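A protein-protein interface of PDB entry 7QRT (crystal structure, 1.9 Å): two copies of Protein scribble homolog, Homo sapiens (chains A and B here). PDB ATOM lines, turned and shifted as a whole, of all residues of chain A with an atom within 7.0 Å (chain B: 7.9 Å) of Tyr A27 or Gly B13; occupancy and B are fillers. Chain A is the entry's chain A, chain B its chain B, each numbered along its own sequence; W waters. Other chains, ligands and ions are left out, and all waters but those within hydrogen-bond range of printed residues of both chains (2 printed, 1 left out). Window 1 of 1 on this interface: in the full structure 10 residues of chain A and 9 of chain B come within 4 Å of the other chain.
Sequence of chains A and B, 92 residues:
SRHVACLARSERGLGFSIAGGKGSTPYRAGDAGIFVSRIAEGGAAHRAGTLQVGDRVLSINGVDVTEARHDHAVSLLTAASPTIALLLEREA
The guanidinium group of Arg B9 is in hydrogen-bond range of the backbone carbonyl oxygen of Tyr A27, at 3.0 Å.
The backbone NH of Gly A54 lies within hydrogen-bond range of the backbone carbonyl oxygen of Val A36 (2.8 Å).
NH1 of Arg B9 lies within hydrogen-bond range of O of Leu B77 (3.3 Å).
NH1 of Arg B9 lies within hydrogen-bond range of O of Ala B80.
NH1 of Arg B9 is in hydrogen-bond range of O of Ser B81 (3.1 Å).
The side-chain carboxylate (OE2) of Glu B11 sits at hydrogen-bond distance from the side-chain hydroxyl (OG) of Ser B10 (2.9 Å).
The guanidinium group (NH2) of Arg B47 is in salt-bridge range of the side-chain carboxylate (OE1) of Glu B11, at 2.7 Å.
Thr A25 touches Ala B80 (CG2 to O, 3.9 Å).
Pro B82 touches Pro A26.
OH of Tyr A27 touches CA of Gly B13, at 3.0 Å.
O of Arg B9 touches CB of Arg A28, at 3.4 Å.
Arg A28 touches Ser B10 (NH1 to C, 3.8 Å).
Arg A28 touches Glu B11 (NH1 to N, 3.5 Å).
Val A53 touches Glu B11 (O to O, 3.6 Å).
CA of Arg B12 touches O of Val A53, 3.5 Å away.
Gly B13 touches Val A53 (CA to CG1, 3.8 Å).
CA of Gly A54 touches O of Glu B11 (3.5 Å).
Tyr A27 touches just these residues of chain B: Arg B9, Gly B13 and Pro B82.
Of chain A, only Tyr A27 and Val A53 come within 4 Å of Gly B13.
Of the printed residues of chain B, Pro A26 touches Pro B82.
Of the printed residues of chain B, Val A53 touches Glu B11 (3.6 Å), Arg B12 (3.5 Å) and Gly B13 (3.8 Å).
Ala B79 touches none of the printed residues of chain A.
The nearest residue of chain B that does not touch Tyr A27 is Ser B10 (4.3 Å).
The nearest residue of chain A that does not touch Gly B13 is Gly A54 (4.1 Å).
The nearest printed residue of chain A that does not touch Pro B82 is Arg A28 (4.1 Å).
Printed residues of chain A that touch a printed residue of chain B: Thr A25, Pro A26, Tyr A27, Arg A28, Ser A37, Val A53 and Gly A54.
Hydrophobic or aromatic side chains of chain A that line the printed part of chain B: Tyr A27 and Val A53.
Along chain A the printed residues that touch a printed residue of chain B span positions 25 to 54.
Printed residues of chain B that touch a printed residue of chain A: Arg B9, Ser B10, Glu B11, Arg B12, Gly B13, Thr B78, Ala B80 and Pro B82.
No position is printed for both chains.
Of the 13 pairs that touch across the chains among the printed residues, none has its exchanged pair printed and touching as well.
Water W1 lies within hydrogen-bond range of NH1 of Arg A28 (2.6 Å), O of Ser B10 (2.9 Å) and O of Gly A54 (3.0 Å).
Water W2 bridges O of Arg B9 (2.7 Å) and N of Ala A29 (3.2 Å).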
ATOM      1  N   ILE A  18     -31.767 -31.368 -18.833  1.00  0.00           N
ATOM      2  CA  ILE A  18     -31.217 -30.169 -18.226  1.00  0.00           C
ATOM      3  C   ILE A  18     -29.809 -30.481 -17.755  1.00  0.00           C
ATOM      4  O   ILE A  18     -29.486 -31.621 -17.418  1.00  0.00           O
ATOM      5  CB  ILE A  18     -32.096 -29.688 -17.056  1.00  0.00           C
ATOM      6  CG1 ILE A  18     -32.264 -30.807 -16.025  1.00  0.00           C
ATOM      7  CG2 ILE A  18     -33.445 -29.248 -17.591  1.00  0.00           C
ATOM      8  CD1 ILE A  18     -32.779 -30.279 -14.703  1.00  0.00           C
ATOM      9  N   ALA A  19     -28.963 -29.467 -17.777  1.00  0.00           N
ATOM     10  CA  ALA A  19     -27.586 -29.596 -17.342  1.00  0.00           C
ATOM     11  C   ALA A  19     -27.204 -28.368 -16.537  1.00  0.00           C
ATOM     12  O   ALA A  19     -27.851 -27.322 -16.611  1.00  0.00           O
ATOM     13  CB  ALA A  19     -26.647 -29.755 -18.537  1.00  0.00           C
ATOM     14  N   GLY A  20     -26.115 -28.496 -15.800  1.00  0.00           N
ATOM     15  CA  GLY A  20     -25.602 -27.392 -15.033  1.00  0.00           C
ATOM     16  C   GLY A  20     -26.083 -27.434 -13.602  1.00  0.00           C
ATOM     17  O   GLY A  20     -26.622 -28.434 -13.119  1.00  0.00           O
ATOM     18  N   GLY A  21     -25.870 -26.319 -12.906  1.00  0.00           N
ATOM     19  CA  GLY A  21     -26.292 -26.245 -11.520  1.00  0.00           C
ATOM     20  C   GLY A  21     -25.162 -25.974 -10.544  1.00  0.00           C
ATOM     21  O   GLY A  21     -23.990 -26.213 -10.853  1.00  0.00           O
ATOM     22  N   SER A  24     -22.038 -28.298  -9.892  1.00  0.00           N
ATOM     23  CA  SER A  24     -21.907 -29.230 -10.995  1.00  0.00           C
ATOM     24  C   SER A  24     -20.975 -28.635 -12.038  1.00  0.00           C
ATOM     25  O   SER A  24     -20.648 -27.442 -12.003  1.00  0.00           O
ATOM     26  CB  SER A  24     -23.283 -29.562 -11.588  1.00  0.00           C
ATOM     27  OG  SER A  24     -24.260 -29.629 -10.559  1.00  0.00           O
ATOM     28  N   THR A  25     -20.495 -29.510 -12.921  1.00  0.00           N
ATOM     29  CA  THR A  25     -19.829 -29.098 -14.144  1.00  0.00           C
ATOM     30  C   THR A  25     -20.686 -28.050 -14.839  1.00  0.00           C
ATOM     31  O   THR A  25     -21.867 -28.314 -15.128  1.00  0.00           O
ATOM     32  CB  THR A  25     -19.665 -30.277 -15.111  1.00  0.00           C
ATOM     33  OG1 THR A  25     -18.971 -31.345 -14.461  1.00  0.00           O
ATOM     34  CG2 THR A  25     -18.949 -29.830 -16.411  1.00  0.00           C
ATOM     35  N   PRO A  26     -20.177 -26.849 -15.082  1.00  0.00           N
ATOM     36  CA  PRO A  26     -21.008 -25.832 -15.721  1.00  0.00           C
ATOM     37  C   PRO A  26     -21.481 -26.306 -17.087  1.00  0.00           C
ATOM     38  O   PRO A  26     -20.751 -26.959 -17.830  1.00  0.00           O
ATOM     39  CB  PRO A  26     -20.078 -24.622 -15.815  1.00  0.00           C
ATOM     40  CG  PRO A  26     -19.100 -24.829 -14.677  1.00  0.00           C
ATOM     41  CD  PRO A  26     -18.924 -26.292 -14.531  1.00  0.00           C
ATOM     42  N   TYR A  27     -22.715 -25.962 -17.435  1.00  0.00           N
ATOM     43  CA  TYR A  27     -23.152 -26.303 -18.781  1.00  0.00           C
ATOM     44  C   TYR A  27     -22.491 -25.416 -19.809  1.00  0.00           C
ATOM     45  O   TYR A  27     -22.246 -25.855 -20.942  1.00  0.00           O
ATOM     46  CB  TYR A  27     -24.662 -26.172 -18.905  1.00  0.00           C
ATOM     47  CG  TYR A  27     -25.173 -26.153 -20.324  1.00  0.00           C
ATOM     48  CD1 TYR A  27     -25.344 -27.335 -21.034  1.00  0.00           C
ATOM     49  CD2 TYR A  27     -25.515 -24.957 -20.946  1.00  0.00           C
ATOM     50  CE1 TYR A  27     -25.842 -27.326 -22.306  1.00  0.00           C
ATOM     51  CE2 TYR A  27     -26.002 -24.941 -22.231  1.00  0.00           C
ATOM     52  CZ  TYR A  27     -26.164 -26.131 -22.904  1.00  0.00           C
ATOM     53  OH  TYR A  27     -26.662 -26.125 -24.186  1.00  0.00           O
ATOM     54  N   ARG A  28     -22.225 -24.167 -19.433  1.00  0.00           N
ATOM     55  CA  ARG A  28     -21.474 -23.208 -20.231  1.00  0.00           C
ATOM     56  C   ARG A  28     -20.531 -22.438 -19.316  1.00  0.00           C
ATOM     57  O   ARG A  28     -20.766 -22.324 -18.106  1.00  0.00           O
ATOM     58  CB  ARG A  28     -22.383 -22.221 -20.967  1.00  0.00           C
ATOM     59  CG  ARG A  28     -23.319 -21.425 -20.069  1.00  0.00           C
ATOM     60  CD  ARG A  28     -24.302 -20.639 -20.907  1.00  0.00           C
ATOM     61  NE  ARG A  28     -23.633 -19.510 -21.531  1.00  0.00           N
ATOM     62  CZ  ARG A  28     -24.242 -18.580 -22.248  1.00  0.00           C
ATOM     63  NH1 ARG A  28     -25.555 -18.635 -22.444  1.00  0.00           N
ATOM     64  NH2 ARG A  28     -23.530 -17.587 -22.766  1.00  0.00           N
ATOM     65  N   ALA A  29     -19.447 -21.926 -19.906  1.00  0.00           N
ATOM     66  CA  ALA A  29     -18.363 -21.329 -19.125  1.00  0.00           C
ATOM     67  C   ALA A  29     -18.850 -20.157 -18.278  1.00  0.00           C
ATOM     68  O   ALA A  29     -19.576 -19.288 -18.763  1.00  0.00           O
ATOM     69  CB  ALA A  29     -17.233 -20.873 -20.055  1.00  0.00           C
ATOM     70  N   ASP A  31     -20.995 -19.825 -15.895  1.00  0.00           N
ATOM     71  CA  ASP A  31     -22.412 -19.730 -15.549  1.00  0.00           C
ATOM     72  C   ASP A  31     -22.817 -21.056 -14.930  1.00  0.00           C
ATOM     73  O   ASP A  31     -22.703 -22.089 -15.594  1.00  0.00           O
ATOM     74  CB  ASP A  31     -23.263 -19.423 -16.775  1.00  0.00           C
ATOM     75  CG  ASP A  31     -24.642 -18.971 -16.412  1.00  0.00           C
ATOM     76  OD1 ASP A  31     -25.090 -17.990 -17.043  1.00  0.00           O
ATOM     77  OD2 ASP A  31     -25.281 -19.594 -15.529  1.00  0.00           O
ATOM     78  N   ALA A  32     -23.183 -21.055 -13.642  1.00  0.00           N
ATOM     79  CA  ALA A  32     -23.589 -22.288 -12.979  1.00  0.00           C
ATOM     80  C   ALA A  32     -25.099 -22.552 -13.067  1.00  0.00           C
ATOM     81  O   ALA A  32     -25.579 -23.498 -12.437  1.00  0.00           O
ATOM     82  CB  ALA A  32     -23.190 -22.269 -11.500  1.00  0.00           C
ATOM     83  N   GLY A  33     -25.823 -21.870 -13.937  1.00  0.00           N
ATOM     84  CA  GLY A  33     -27.261 -22.062 -13.982  1.00  0.00           C
ATOM     85  C   GLY A  33     -27.635 -23.430 -14.553  1.00  0.00           C
ATOM     86  O   GLY A  33     -26.797 -24.239 -14.956  1.00  0.00           O
ATOM     87  N   ILE A  34     -28.946 -23.690 -14.521  1.00  0.00           N
ATOM     88  CA  ILE A  34     -29.572 -24.880 -15.081  1.00  0.00           C
ATOM     89  C   ILE A  34     -30.068 -24.525 -16.470  1.00  0.00           C
ATOM     90  O   ILE A  34     -30.789 -23.534 -16.645  1.00  0.00           O
ATOM     91  CB  ILE A  34     -30.746 -25.357 -14.209  1.00  0.00           C
ATOM     92  CG1 ILE A  34     -30.309 -25.443 -12.745  1.00  0.00           C
ATOM     93  CG2 ILE A  34     -31.308 -26.647 -14.776  1.00  0.00           C
ATOM     94  CD1 ILE A  34     -29.786 -26.751 -12.339  1.00  0.00           C
ATOM     95  N   PHE A  35     -29.701 -25.327 -17.458  1.00  0.00           N
ATOM     96  CA  PHE A  35     -30.041 -25.031 -18.840  1.00  0.00           C
ATOM     97  C   PHE A  35     -30.621 -26.252 -19.534  1.00  0.00           C
ATOM     98  O   PHE A  35     -30.238 -27.382 -19.234  1.00  0.00           O
ATOM     99  CB  PHE A  35     -28.793 -24.591 -19.617  1.00  0.00           C
ATOM    100  CG  PHE A  35     -28.170 -23.314 -19.137  1.00  0.00           C
ATOM    101  CD1 PHE A  35     -27.195 -23.315 -18.143  1.00  0.00           C
ATOM    102  CD2 PHE A  35     -28.513 -22.115 -19.725  1.00  0.00           C
ATOM    103  CE1 PHE A  35     -26.601 -22.136 -17.731  1.00  0.00           C
ATOM    104  CE2 PHE A  35     -27.927 -20.933 -19.315  1.00  0.00           C
ATOM    105  CZ  PHE A  35     -26.965 -20.945 -18.313  1.00  0.00           C
ATOM    106  N   VAL A  36     -31.483 -26.017 -20.521  1.00  0.00           N
ATOM    107  CA  VAL A  36     -31.938 -27.100 -21.399  1.00  0.00           C
ATOM    108  C   VAL A  36     -30.764 -27.476 -22.306  1.00  0.00           C
ATOM    109  O   VAL A  36     -30.177 -26.614 -22.966  1.00  0.00           O
ATOM    110  CB  VAL A  36     -33.158 -26.688 -22.227  1.00  0.00           C
ATOM    111  CG1 VAL A  36     -33.547 -27.850 -23.161  1.00  0.00           C
ATOM    112  CG2 VAL A  36     -34.332 -26.260 -21.344  1.00  0.00           C
ATOM    113  N   SER A  37     -30.362 -28.739 -22.267  1.00  0.00           N
ATOM    114  CA  SER A  37     -29.120 -29.162 -22.907  1.00  0.00           C
ATOM    115  C   SER A  37     -29.269 -29.973 -24.191  1.00  0.00           C
ATOM    116  O   SER A  37     -28.270 -30.178 -24.891  1.00  0.00           O
ATOM    117  CB  SER A  37     -28.294 -29.989 -21.926  1.00  0.00           C
ATOM    118  OG  SER A  37     -29.075 -31.039 -21.373  1.00  0.00           O
ATOM    119  N   ARG A  38     -30.427 -30.562 -24.431  1.00  0.00           N
ATOM    120  CA  ARG A  38     -30.652 -31.368 -25.610  1.00  0.00           C
ATOM    121  C   ARG A  38     -32.156 -31.348 -25.868  1.00  0.00           C
ATOM    122  O   ARG A  38     -32.950 -31.342 -24.918  1.00  0.00           O
ATOM    123  CB  ARG A  38     -30.166 -32.811 -25.381  1.00  0.00           C
ATOM    124  CG  ARG A  38     -31.220 -33.561 -24.634  1.00  0.00           C
ATOM    125  CD  ARG A  38     -31.226 -35.064 -24.806  1.00  0.00           C
ATOM    126  NE  ARG A  38     -32.227 -35.606 -23.885  1.00  0.00           N
ATOM    127  CZ  ARG A  38     -33.267 -36.360 -24.196  1.00  0.00           C
ATOM    128  NH1 ARG A  38     -34.080 -36.740 -23.215  1.00  0.00           N
ATOM    129  NH2 ARG A  38     -33.468 -36.810 -25.433  1.00  0.00           N
ATOM    130  N   VAL A  53     -32.759 -25.382 -26.921  1.00  0.00           N
ATOM    131  CA  VAL A  53     -31.496 -25.722 -26.296  1.00  0.00           C
ATOM    132  C   VAL A  53     -30.775 -24.446 -25.902  1.00  0.00           C
ATOM    133  O   VAL A  53     -30.735 -23.470 -26.662  1.00  0.00           O
ATOM    134  CB  VAL A  53     -30.629 -26.581 -27.227  1.00  0.00           C
ATOM    135  CG1 VAL A  53     -29.216 -26.656 -26.668  1.00  0.00           C
ATOM    136  CG2 VAL A  53     -31.214 -27.965 -27.340  1.00  0.00           C
ATOM    137  N   GLY A  54     -30.233 -24.444 -24.687  1.00  0.00           N
ATOM    138  CA  GLY A  54     -29.565 -23.294 -24.138  1.00  0.00           C
ATOM    139  C   GLY A  54     -30.451 -22.390 -23.305  1.00  0.00           C
ATOM    140  O   GLY A  54     -29.936 -21.466 -22.654  1.00  0.00           O
ATOM    141  N   ASP A  55     -31.759 -22.589 -23.342  1.00  0.00           N
ATOM    142  CA  ASP A  55     -32.654 -21.852 -22.458  1.00  0.00           C
ATOM    143  C   ASP A  55     -32.235 -22.089 -21.007  1.00  0.00           C
ATOM    144  O   ASP A  55     -31.920 -23.219 -20.616  1.00  0.00           O
ATOM    145  CB  ASP A  55     -34.096 -22.304 -22.675  1.00  0.00           C
ATOM    146  CG  ASP A  55     -34.732 -21.723 -23.926  1.00  0.00           C
ATOM    147  OD1 ASP A  55     -34.114 -20.855 -24.593  1.00  0.00           O
ATOM    148  OD2 ASP A  55     -35.870 -22.145 -24.250  1.00  0.00           O
ATOM    149  N   LEU B   7     -15.937 -26.253 -30.395  1.00  0.00           N
ATOM    150  CA  LEU B   7     -17.096 -25.425 -30.101  1.00  0.00           C
ATOM    151  C   LEU B   7     -17.313 -25.305 -28.606  1.00  0.00           C
ATOM    152  O   LEU B   7     -17.203 -26.297 -27.878  1.00  0.00           O
ATOM    153  CB  LEU B   7     -18.385 -25.996 -30.731  1.00  0.00           C
ATOM    154  CG  LEU B   7     -18.561 -26.092 -32.242  1.00  0.00           C
ATOM    155  CD1 LEU B   7     -19.849 -26.836 -32.603  1.00  0.00           C
ATOM    156  CD2 LEU B   7     -18.558 -24.683 -32.803  1.00  0.00           C
ATOM    157  N   ALA B   8     -17.615 -24.098 -28.143  1.00  0.00           N
ATOM    158  CA  ALA B   8     -17.980 -23.873 -26.749  1.00  0.00           C
ATOM    159  C   ALA B   8     -19.496 -23.711 -26.640  1.00  0.00           C
ATOM    160  O   ALA B   8     -20.097 -22.951 -27.406  1.00  0.00           O
ATOM    161  CB  ALA B   8     -17.282 -22.636 -26.192  1.00  0.00           C
ATOM    162  N   ARG B   9     -20.103 -24.386 -25.667  1.00  0.00           N
ATOM    163  CA  ARG B   9     -21.549 -24.276 -25.491  1.00  0.00           C
ATOM    164  C   ARG B   9     -21.902 -22.856 -25.067  1.00  0.00           C
ATOM    165  O   ARG B   9     -21.227 -22.267 -24.216  1.00  0.00           O
ATOM    166  CB  ARG B   9     -22.070 -25.227 -24.410  1.00  0.00           C
ATOM    167  CG  ARG B   9     -22.039 -26.691 -24.696  1.00  0.00           C
ATOM    168  CD  ARG B   9     -22.887 -27.460 -23.666  1.00  0.00           C
ATOM    169  NE  ARG B   9     -22.405 -28.829 -23.593  1.00  0.00           N
ATOM    170  CZ  ARG B   9     -21.783 -29.380 -22.555  1.00  0.00           C
ATOM    171  NH1 ARG B   9     -21.382 -30.641 -22.652  1.00  0.00           N
ATOM    172  NH2 ARG B   9     -21.589 -28.708 -21.423  1.00  0.00           N
ATOM    173  N   SER B  10     -22.924 -22.292 -25.705  1.00  0.00           N
ATOM    174  CA  SER B  10     -23.316 -20.906 -25.483  1.00  0.00           C
ATOM    175  C   SER B  10     -24.845 -20.828 -25.486  1.00  0.00           C
ATOM    176  O   SER B  10     -25.547 -21.777 -25.117  1.00  0.00           O
ATOM    177  CB  SER B  10     -22.617 -19.992 -26.503  1.00  0.00           C
ATOM    178  OG  SER B  10     -22.986 -20.338 -27.813  1.00  0.00           O
ATOM    179  N   GLU B  11     -25.375 -19.646 -25.805  1.00  0.00           N
ATOM    180  CA  GLU B  11     -26.811 -19.374 -25.671  1.00  0.00           C
ATOM    181  C   GLU B  11     -27.715 -20.357 -26.414  1.00  0.00           C
ATOM    182  O   GLU B  11     -28.900 -20.466 -26.080  1.00  0.00           O
ATOM    183  CB  GLU B  11     -27.085 -17.934 -26.107  1.00  0.00           C
ATOM    184  CG  GLU B  11     -27.075 -17.685 -27.600  1.00  0.00           C
ATOM    185  CD  GLU B  11     -25.698 -17.774 -28.273  1.00  0.00           C
ATOM    186  OE1 GLU B  11     -25.657 -17.638 -29.516  1.00  0.00           O
ATOM    187  OE2 GLU B  11     -24.668 -17.965 -27.593  1.00  0.00           O
ATOM    188  N   ARG B  12     -27.251 -20.931 -27.521  1.00  0.00           N
ATOM    189  CA  ARG B  12     -27.994 -21.975 -28.216  1.00  0.00           C
ATOM    190  C   ARG B  12     -27.370 -23.349 -28.009  1.00  0.00           C
ATOM    191  O   ARG B  12     -27.622 -24.277 -28.787  1.00  0.00           O
ATOM    192  CB  ARG B  12     -28.134 -21.600 -29.692  1.00  0.00           C
ATOM    193  CG  ARG B  12     -28.974 -20.316 -29.833  1.00  0.00           C
ATOM    194  CD  ARG B  12     -29.867 -20.307 -31.051  1.00  0.00           C
ATOM    195  NE  ARG B  12     -30.601 -21.557 -31.210  1.00  0.00           N
ATOM    196  CZ  ARG B  12     -31.410 -21.816 -32.230  1.00  0.00           C
ATOM    197  NH1 ARG B  12     -31.585 -20.904 -33.175  1.00  0.00           N
ATOM    198  NH2 ARG B  12     -32.041 -22.980 -32.306  1.00  0.00           N
ATOM    199  N   GLY B  13     -26.612 -23.523 -26.930  1.00  0.00           N
ATOM    200  CA  GLY B  13     -25.886 -24.767 -26.777  1.00  0.00           C
ATOM    201  C   GLY B  13     -24.748 -24.763 -27.780  1.00  0.00           C
ATOM    202  O   GLY B  13     -24.064 -23.754 -27.968  1.00  0.00           O
ATOM    203  N   LEU B  14     -24.496 -25.931 -28.376  1.00  0.00           N
ATOM    204  CA  LEU B  14     -23.558 -26.039 -29.485  1.00  0.00           C
ATOM    205  C   LEU B  14     -24.156 -25.454 -30.757  1.00  0.00           C
ATOM    206  O   LEU B  14     -23.425 -25.014 -31.659  1.00  0.00           O
ATOM    207  CB  LEU B  14     -23.176 -27.495 -29.686  1.00  0.00           C
ATOM    208  CG  LEU B  14     -22.577 -28.227 -28.491  1.00  0.00           C
ATOM    209  CD1 LEU B  14     -22.327 -29.677 -28.870  1.00  0.00           C
ATOM    210  CD2 LEU B  14     -21.313 -27.479 -28.099  1.00  0.00           C
ATOM    211  N   GLY B  15     -25.474 -25.491 -30.865  1.00  0.00           N
ATOM    212  CA  GLY B  15     -26.155 -24.866 -31.976  1.00  0.00           C
ATOM    213  C   GLY B  15     -26.163 -25.677 -33.250  1.00  0.00           C
ATOM    214  O   GLY B  15     -26.070 -25.106 -34.344  1.00  0.00           O
ATOM    215  N   PHE B  16     -26.272 -26.999 -33.135  1.00  0.00           N
ATOM    216  CA  PHE B  16     -26.451 -27.874 -34.286  1.00  0.00           C
ATOM    217  C   PHE B  16     -27.196 -29.112 -33.808  1.00  0.00           C
ATOM    218  O   PHE B  16     -27.461 -29.298 -32.612  1.00  0.00           O
ATOM    219  CB  PHE B  16     -25.108 -28.199 -35.017  1.00  0.00           C
ATOM    220  CG  PHE B  16     -24.151 -29.114 -34.263  1.00  0.00           C
ATOM    221  CD1 PHE B  16     -24.047 -30.457 -34.584  1.00  0.00           C
ATOM    222  CD2 PHE B  16     -23.316 -28.610 -33.268  1.00  0.00           C
ATOM    223  CE1 PHE B  16     -23.159 -31.289 -33.897  1.00  0.00           C
ATOM    224  CE2 PHE B  16     -22.437 -29.437 -32.574  1.00  0.00           C
ATOM    225  CZ  PHE B  16     -22.358 -30.773 -32.889  1.00  0.00           C
ATOM    226  N   GLY B  42     -28.471 -19.125 -35.479  1.00  0.00           N
ATOM    227  CA  GLY B  42     -27.734 -18.470 -34.410  1.00  0.00           C
ATOM    228  C   GLY B  42     -26.987 -19.481 -33.557  1.00  0.00           C
ATOM    229  O   GLY B  42     -27.356 -20.657 -33.524  1.00  0.00           O
ATOM    230  N   GLY B  43     -25.954 -19.079 -32.840  1.00  0.00           N
ATOM    231  CA  GLY B  43     -25.292 -20.010 -31.950  1.00  0.00           C
ATOM    232  C   GLY B  43     -23.858 -20.286 -32.346  1.00  0.00           C
ATOM    233  O   GLY B  43     -23.346 -19.801 -33.355  1.00  0.00           O
ATOM    234  N   ALA B  44     -23.213 -21.102 -31.519  1.00  0.00           N
ATOM    235  CA  ALA B  44     -21.773 -21.286 -31.644  1.00  0.00           C
ATOM    236  C   ALA B  44     -21.382 -21.921 -32.967  1.00  0.00           C
ATOM    237  O   ALA B  44     -20.448 -21.460 -33.635  1.00  0.00           O
ATOM    238  CB  ALA B  44     -21.261 -22.138 -30.488  1.00  0.00           C
ATOM    239  N   ALA B  45     -22.050 -23.008 -33.352  1.00  0.00           N
ATOM    240  CA  ALA B  45     -21.655 -23.678 -34.584  1.00  0.00           C
ATOM    241  C   ALA B  45     -21.762 -22.723 -35.758  1.00  0.00           C
ATOM    242  O   ALA B  45     -20.920 -22.740 -36.663  1.00  0.00           O
ATOM    243  CB  ALA B  45     -22.513 -24.921 -34.828  1.00  0.00           C
ATOM    244  N   ARG B  47     -21.520 -19.374 -35.694  1.00  0.00           N
ATOM    245  CA  ARG B  47     -20.445 -18.392 -35.682  1.00  0.00           C
ATOM    246  C   ARG B  47     -19.105 -19.011 -36.075  1.00  0.00           C
ATOM    247  O   ARG B  47     -18.278 -18.334 -36.689  1.00  0.00           O
ATOM    248  CB  ARG B  47     -20.347 -17.744 -34.306  1.00  0.00           C
ATOM    249  CG  ARG B  47     -21.584 -16.960 -33.929  1.00  0.00           C
ATOM    250  CD  ARG B  47     -21.367 -16.198 -32.643  1.00  0.00           C
ATOM    251  NE  ARG B  47     -21.262 -17.086 -31.494  1.00  0.00           N
ATOM    252  CZ  ARG B  47     -22.280 -17.409 -30.701  1.00  0.00           C
ATOM    253  NH1 ARG B  47     -22.079 -18.227 -29.676  1.00  0.00           N
ATOM    254  NH2 ARG B  47     -23.491 -16.914 -30.924  1.00  0.00           N
ATOM    255  N   LEU B  77     -21.926 -35.102 -26.246  1.00  0.00           N
ATOM    256  CA  LEU B  77     -22.046 -33.698 -26.635  1.00  0.00           C
ATOM    257  C   LEU B  77     -22.611 -32.794 -25.558  1.00  0.00           C
ATOM    258  O   LEU B  77     -22.455 -31.565 -25.642  1.00  0.00           O
ATOM    259  CB  LEU B  77     -22.917 -33.569 -27.879  1.00  0.00           C
ATOM    260  CG  LEU B  77     -22.331 -34.278 -29.094  1.00  0.00           C
ATOM    261  CD1 LEU B  77     -23.456 -34.513 -30.084  1.00  0.00           C
ATOM    262  CD2 LEU B  77     -21.203 -33.472 -29.703  1.00  0.00           C
ATOM    263  N   THR B  78     -23.401 -33.344 -24.647  1.00  0.00           N
ATOM    264  CA  THR B  78     -24.120 -32.519 -23.690  1.00  0.00           C
ATOM    265  C   THR B  78     -23.818 -32.800 -22.229  1.00  0.00           C
ATOM    266  O   THR B  78     -24.176 -31.972 -21.385  1.00  0.00           O
ATOM    267  CB  THR B  78     -25.637 -32.690 -23.897  1.00  0.00           C
ATOM    268  OG1 THR B  78     -25.984 -34.065 -23.667  1.00  0.00           O
ATOM    269  CG2 THR B  78     -26.046 -32.328 -25.310  1.00  0.00           C
ATOM    270  N   ALA B  79     -23.229 -33.943 -21.896  1.00  0.00           N
ATOM    271  CA  ALA B  79     -22.993 -34.286 -20.503  1.00  0.00           C
ATOM    272  C   ALA B  79     -21.540 -34.183 -20.047  1.00  0.00           C
ATOM    273  O   ALA B  79     -21.250 -34.551 -18.905  1.00  0.00           O
ATOM    274  CB  ALA B  79     -23.506 -35.703 -20.231  1.00  0.00           C
ATOM    275  N   ALA B  80     -20.619 -33.713 -20.885  1.00  0.00           N
ATOM    276  CA  ALA B  80     -19.219 -33.592 -20.511  1.00  0.00           C
ATOM    277  C   ALA B  80     -18.814 -32.120 -20.433  1.00  0.00           C
ATOM    278  O   ALA B  80     -19.612 -31.275 -19.993  1.00  0.00           O
ATOM    279  CB  ALA B  80     -18.371 -34.410 -21.490  1.00  0.00           C
ATOM    280  N   SER B  81     -17.594 -31.815 -20.860  1.00  0.00           N
ATOM    281  CA  SER B  81     -17.077 -30.458 -20.789  1.00  0.00           C
ATOM    282  C   SER B  81     -17.844 -29.526 -21.731  1.00  0.00           C
ATOM    283  O   SER B  81     -18.338 -29.951 -22.783  1.00  0.00           O
ATOM    284  CB  SER B  81     -15.589 -30.449 -21.132  1.00  0.00           C
ATOM    285  OG  SER B  81     -15.225 -29.242 -21.780  1.00  0.00           O
ATOM    286  N   PRO B  82     -17.952 -28.240 -21.375  1.00  0.00           N
ATOM    287  CA  PRO B  82     -18.633 -27.288 -22.262  1.00  0.00           C
ATOM    288  C   PRO B  82     -17.912 -27.073 -23.582  1.00  0.00           C
ATOM    289  O   PRO B  82     -18.552 -26.619 -24.538  1.00  0.00           O
ATOM    290  CB  PRO B  82     -18.668 -25.990 -21.438  1.00  0.00           C
ATOM    291  CG  PRO B  82     -18.497 -26.414 -20.006  1.00  0.00           C
ATOM    292  CD  PRO B  82     -17.664 -27.660 -20.047  1.00  0.00           C
ATOM    293  N   THR B  83     -16.630 -27.421 -23.698  1.00  0.00           N
ATOM    294  CA  THR B  83     -15.910 -27.251 -24.953  1.00  0.00           C
ATOM    295  C   THR B  83     -15.890 -28.606 -25.651  1.00  0.00           C
ATOM    296  O   THR B  83     -15.523 -29.625 -25.049  1.00  0.00           O
ATOM    297  CB  THR B  83     -14.480 -26.742 -24.743  1.00  0.00           C
ATOM    298  OG1 THR B  83     -14.513 -25.517 -24.003  1.00  0.00           O
ATOM    299  CG2 THR B  83     -13.789 -26.496 -26.091  1.00  0.00           C
HETATM  300  O   HOH W   1     -26.971 -20.855 -22.740  1.00  0.00           O
HETATM  301  O   HOH W   2     -18.877 -22.712 -22.912  1.00  0.00           O
